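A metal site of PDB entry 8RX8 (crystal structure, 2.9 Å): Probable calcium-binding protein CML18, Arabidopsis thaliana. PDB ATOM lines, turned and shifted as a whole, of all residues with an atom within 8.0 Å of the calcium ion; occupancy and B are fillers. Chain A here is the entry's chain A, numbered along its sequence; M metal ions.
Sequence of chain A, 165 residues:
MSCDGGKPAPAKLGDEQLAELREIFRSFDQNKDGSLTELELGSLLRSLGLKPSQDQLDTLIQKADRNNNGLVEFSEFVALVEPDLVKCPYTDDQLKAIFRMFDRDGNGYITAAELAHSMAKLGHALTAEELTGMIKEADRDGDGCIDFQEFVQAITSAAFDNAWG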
ATOM      1  N   PHE A  99      -9.269 -32.017  -0.949  1.00  0.00           N
ATOM      2  CA  PHE A  99      -9.579 -30.819  -0.171  1.00  0.00           C
ATOM      3  C   PHE A  99     -10.979 -30.345  -0.527  1.00  0.00           C
ATOM      4  O   PHE A  99     -11.649 -29.701   0.299  1.00  0.00           O
ATOM      5  CB  PHE A  99      -8.545 -29.739  -0.449  1.00  0.00           C
ATOM      6  CG  PHE A  99      -8.896 -28.391   0.121  1.00  0.00           C
ATOM      7  CD1 PHE A  99      -8.510 -28.045   1.400  1.00  0.00           C
ATOM      8  CD2 PHE A  99      -9.606 -27.468  -0.627  1.00  0.00           C
ATOM      9  CE1 PHE A  99      -8.825 -26.804   1.924  1.00  0.00           C
ATOM     10  CE2 PHE A  99      -9.930 -26.228  -0.108  1.00  0.00           C
ATOM     11  CZ  PHE A  99      -9.538 -25.900   1.166  1.00  0.00           C
ATOM     12  N   PHE A 102     -13.304 -32.321   1.466  1.00  0.00           N
ATOM     13  CA  PHE A 102     -13.368 -31.878   2.863  1.00  0.00           C
ATOM     14  C   PHE A 102     -14.096 -30.550   3.015  1.00  0.00           C
ATOM     15  O   PHE A 102     -15.049 -30.445   3.781  1.00  0.00           O
ATOM     16  CB  PHE A 102     -11.980 -31.763   3.484  1.00  0.00           C
ATOM     17  CG  PHE A 102     -11.474 -33.031   4.115  1.00  0.00           C
ATOM     18  CD1 PHE A 102     -10.854 -34.016   3.367  1.00  0.00           C
ATOM     19  CD2 PHE A 102     -11.622 -33.214   5.486  1.00  0.00           C
ATOM     20  CE1 PHE A 102     -10.412 -35.169   3.978  1.00  0.00           C
ATOM     21  CE2 PHE A 102     -11.174 -34.365   6.088  1.00  0.00           C
ATOM     22  CZ  PHE A 102     -10.565 -35.341   5.337  1.00  0.00           C
ATOM     23  N   ASP A 103     -13.650 -29.524   2.290  1.00  0.00           N
ATOM     24  CA  ASP A 103     -14.345 -28.248   2.288  1.00  0.00           C
ATOM     25  C   ASP A 103     -15.640 -28.419   1.516  1.00  0.00           C
ATOM     26  O   ASP A 103     -15.676 -28.248   0.296  1.00  0.00           O
ATOM     27  CB  ASP A 103     -13.470 -27.146   1.695  1.00  0.00           C
ATOM     28  CG  ASP A 103     -14.126 -25.784   1.744  1.00  0.00           C
ATOM     29  OD1 ASP A 103     -15.100 -25.618   2.494  1.00  0.00           O
ATOM     30  OD2 ASP A 103     -13.641 -24.868   1.037  1.00  0.00           O
ATOM     31  N   ARG A 104     -16.724 -28.766   2.221  1.00  0.00           N
ATOM     32  CA  ARG A 104     -17.969 -29.055   1.522  1.00  0.00           C
ATOM     33  C   ARG A 104     -18.589 -27.781   0.944  1.00  0.00           C
ATOM     34  O   ARG A 104     -19.067 -27.781  -0.188  1.00  0.00           O
ATOM     35  CB  ARG A 104     -18.934 -29.801   2.460  1.00  0.00           C
ATOM     36  CG  ARG A 104     -20.044 -28.985   3.123  1.00  0.00           C
ATOM     37  CD  ARG A 104     -19.663 -28.600   4.554  1.00  0.00           C
ATOM     38  NE  ARG A 104     -19.761 -27.181   4.802  1.00  0.00           N
ATOM     39  CZ  ARG A 104     -20.577 -26.577   5.665  1.00  0.00           C
ATOM     40  NH1 ARG A 104     -20.622 -26.941   6.928  1.00  0.00           N
ATOM     41  NH2 ARG A 104     -21.193 -25.453   5.295  1.00  0.00           N
ATOM     42  N   ASP A 105     -18.574 -26.686   1.708  1.00  0.00           N
ATOM     43  CA  ASP A 105     -19.103 -25.423   1.212  1.00  0.00           C
ATOM     44  C   ASP A 105     -18.212 -24.809   0.143  1.00  0.00           C
ATOM     45  O   ASP A 105     -18.594 -23.789  -0.457  1.00  0.00           O
ATOM     46  CB  ASP A 105     -19.336 -24.456   2.369  1.00  0.00           C
ATOM     47  CG  ASP A 105     -18.221 -23.457   2.522  1.00  0.00           C
ATOM     48  OD1 ASP A 105     -17.178 -23.812   3.120  1.00  0.00           O
ATOM     49  OD2 ASP A 105     -18.391 -22.318   2.052  1.00  0.00           O
ATOM     50  N   GLY A 106     -17.067 -25.423  -0.130  1.00  0.00           N
ATOM     51  CA  GLY A 106     -16.155 -24.977  -1.179  1.00  0.00           C
ATOM     52  C   GLY A 106     -15.759 -23.520  -1.168  1.00  0.00           C
ATOM     53  O   GLY A 106     -15.615 -22.914  -2.237  1.00  0.00           O
ATOM     54  N   ASN A 107     -15.583 -22.939   0.014  1.00  0.00           N
ATOM     55  CA  ASN A 107     -15.149 -21.540   0.102  1.00  0.00           C
ATOM     56  C   ASN A 107     -13.643 -21.394   0.151  1.00  0.00           C
ATOM     57  O   ASN A 107     -13.153 -20.265   0.279  1.00  0.00           O
ATOM     58  CB  ASN A 107     -15.750 -20.859   1.337  1.00  0.00           C
ATOM     59  CG  ASN A 107     -15.440 -21.604   2.630  1.00  0.00           C
ATOM     60  OD1 ASN A 107     -14.546 -22.458   2.674  1.00  0.00           O
ATOM     61  ND2 ASN A 107     -16.165 -21.283   3.692  1.00  0.00           N
ATOM     62  N   GLY A 108     -12.886 -22.491   0.052  1.00  0.00           N
ATOM     63  CA  GLY A 108     -11.443 -22.427   0.150  1.00  0.00           C
ATOM     64  C   GLY A 108     -10.886 -22.599   1.545  1.00  0.00           C
ATOM     65  O   GLY A 108      -9.656 -22.569   1.702  1.00  0.00           O
ATOM     66  N   TYR A 109     -11.731 -22.783   2.557  1.00  0.00           N
ATOM     67  CA  TYR A 109     -11.280 -22.982   3.932  1.00  0.00           C
ATOM     68  C   TYR A 109     -12.035 -24.141   4.558  1.00  0.00           C
ATOM     69  O   TYR A 109     -13.244 -24.296   4.363  1.00  0.00           O
ATOM     70  CB  TYR A 109     -11.497 -21.718   4.776  1.00  0.00           C
ATOM     71  CG  TYR A 109     -10.686 -20.516   4.321  1.00  0.00           C
ATOM     72  CD1 TYR A 109     -11.147 -19.694   3.303  1.00  0.00           C
ATOM     73  CD2 TYR A 109      -9.465 -20.221   4.916  1.00  0.00           C
ATOM     74  CE1 TYR A 109     -10.415 -18.599   2.890  1.00  0.00           C
ATOM     75  CE2 TYR A 109      -8.718 -19.131   4.499  1.00  0.00           C
ATOM     76  CZ  TYR A 109      -9.197 -18.317   3.491  1.00  0.00           C
ATOM     77  OH  TYR A 109      -8.463 -17.232   3.076  1.00  0.00           O
ATOM     78  N   ILE A 110     -11.304 -24.964   5.311  1.00  0.00           N
ATOM     79  CA  ILE A 110     -11.886 -26.068   6.065  1.00  0.00           C
ATOM     80  C   ILE A 110     -12.126 -25.577   7.490  1.00  0.00           C
ATOM     81  O   ILE A 110     -11.184 -25.426   8.270  1.00  0.00           O
ATOM     82  CB  ILE A 110     -10.974 -27.298   6.053  1.00  0.00           C
ATOM     83  CG1 ILE A 110     -10.806 -27.821   4.630  1.00  0.00           C
ATOM     84  CG2 ILE A 110     -11.545 -28.397   6.945  1.00  0.00           C
ATOM     85  CD1 ILE A 110      -9.884 -29.022   4.548  1.00  0.00           C
ATOM     86  N   THR A 111     -13.393 -25.343   7.828  1.00  0.00           N
ATOM     87  CA  THR A 111     -13.731 -24.973   9.187  1.00  0.00           C
ATOM     88  C   THR A 111     -13.630 -26.180  10.118  1.00  0.00           C
ATOM     89  O   THR A 111     -13.548 -27.338   9.675  1.00  0.00           O
ATOM     90  CB  THR A 111     -15.151 -24.386   9.261  1.00  0.00           C
ATOM     91  OG1 THR A 111     -16.081 -25.416   9.643  1.00  0.00           O
ATOM     92  CG2 THR A 111     -15.561 -23.819   7.915  1.00  0.00           C
ATOM     93  N   ALA A 112     -13.614 -25.907  11.421  1.00  0.00           N
ATOM     94  CA  ALA A 112     -13.680 -26.994  12.405  1.00  0.00           C
ATOM     95  C   ALA A 112     -14.976 -27.774  12.272  1.00  0.00           C
ATOM     96  O   ALA A 112     -15.009 -28.981  12.537  1.00  0.00           O
ATOM     97  CB  ALA A 112     -13.531 -26.438  13.815  1.00  0.00           C
ATOM     98  N   ALA A 113     -16.063 -27.110  11.863  1.00  0.00           N
ATOM     99  CA  ALA A 113     -17.325 -27.799  11.650  1.00  0.00           C
ATOM    100  C   ALA A 113     -17.227 -28.758  10.470  1.00  0.00           C
ATOM    101  O   ALA A 113     -17.637 -29.922  10.560  1.00  0.00           O
ATOM    102  CB  ALA A 113     -18.440 -26.789  11.419  1.00  0.00           C
ATOM    103  N   GLU A 114     -16.678 -28.288   9.351  1.00  0.00           N
ATOM    104  CA  GLU A 114     -16.495 -29.152   8.191  1.00  0.00           C
ATOM    105  C   GLU A 114     -15.532 -30.287   8.497  1.00  0.00           C
ATOM    106  O   GLU A 114     -15.765 -31.429   8.090  1.00  0.00           O
ATOM    107  CB  GLU A 114     -15.985 -28.345   6.994  1.00  0.00           C
ATOM    108  CG  GLU A 114     -16.872 -27.181   6.612  1.00  0.00           C
ATOM    109  CD  GLU A 114     -16.358 -26.472   5.377  1.00  0.00           C
ATOM    110  OE1 GLU A 114     -15.119 -26.358   5.217  1.00  0.00           O
ATOM    111  OE2 GLU A 114     -17.197 -26.038   4.554  1.00  0.00           O
ATOM    112  N   LEU A 115     -14.442 -29.995   9.220  1.00  0.00           N
ATOM    113  CA  LEU A 115     -13.484 -31.046   9.571  1.00  0.00           C
ATOM    114  C   LEU A 115     -14.139 -32.096  10.465  1.00  0.00           C
ATOM    115  O   LEU A 115     -13.912 -33.302  10.292  1.00  0.00           O
ATOM    116  CB  LEU A 115     -12.264 -30.439  10.245  1.00  0.00           C
ATOM    117  CG  LEU A 115     -11.152 -31.434  10.596  1.00  0.00           C
ATOM    118  CD1 LEU A 115     -10.756 -32.206   9.351  1.00  0.00           C
ATOM    119  CD2 LEU A 115      -9.949 -30.711  11.205  1.00  0.00           C
ATOM    120  N   CYS A 145      -9.301 -21.909  10.566  1.00  0.00           N
ATOM    121  CA  CYS A 145      -9.651 -22.875   9.538  1.00  0.00           C
ATOM    122  C   CYS A 145      -8.378 -23.408   8.874  1.00  0.00           C
ATOM    123  O   CYS A 145      -7.261 -23.208   9.372  1.00  0.00           O
ATOM    124  CB  CYS A 145     -10.601 -22.230   8.523  1.00  0.00           C
ATOM    125  SG  CYS A 145     -11.018 -20.502   8.875  1.00  0.00           S
ATOM    126  N   ILE A 146      -8.537 -24.083   7.753  1.00  0.00           N
ATOM    127  CA  ILE A 146      -7.415 -24.704   7.039  1.00  0.00           C
ATOM    128  C   ILE A 146      -7.629 -24.453   5.553  1.00  0.00           C
ATOM    129  O   ILE A 146      -8.638 -24.882   4.982  1.00  0.00           O
ATOM    130  CB  ILE A 146      -7.324 -26.217   7.311  1.00  0.00           C
ATOM    131  CG1 ILE A 146      -6.867 -26.473   8.756  1.00  0.00           C
ATOM    132  CG2 ILE A 146      -6.379 -26.882   6.318  1.00  0.00           C
ATOM    133  CD1 ILE A 146      -6.806 -27.928   9.108  1.00  0.00           C
HETATM  134 CA    CA M   1     -15.774 -23.837   4.934  1.00  0.00          CA
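CG2 of Thr 111 touches the calcium ion (3.0 Å). Within 4 Å of the calcium ion: Asp 103, Asp 105, Asn 107, Tyr 109, Thr 111 and Glu 114.
The side-chain hydroxyl of Thr 111 lies within hydrogen-bond range of the backbone NH of Ala 113. The backbone NH of Tyr 109 sits at hydrogen-bond distance from the side-chain carboxylate of Asp 103 (3.2 Å). N of Asn 107 sits at hydrogen-bond distance from OD2 of Asp 103 (2.9 Å). The side-chain carboxylate (OD1) of Asp 103 sits at hydrogen-bond distance from the backbone NH (N) of Gly 106 (3.3 Å). OD2 of Asp 103 is in hydrogen-bond range of N of Gly 108 (2.7 Å). OE2 of Glu 114 lies close to NE of Arg 104, at 2.8 Å. The backbone NH (N) of Glu 114 sits at hydrogen-bond distance from the side-chain hydroxyl (OG1) of Thr 111 (2.9 Å).
OD1 of Asp 105 binds the calcium ion (2.3 Å). OE1 of Glu 114 binds the calcium ion, at 2.6 Å. O of Tyr 109 is bound to the calcium ion (2.6 Å). The calcium ion is bound by the side-chain carboxylate (OE2) of Glu 114 (2.6 Å). The calcium ion is bound by the side-chain amide nitrogen (ND2) of Asn 107, at 2.9 Å. OD1 of Asn 107 is bound to the calcium ion, 2.9 Å away. Slightly farther from the calcium ion lies OD1 of Asp 103 (3.1 Å).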
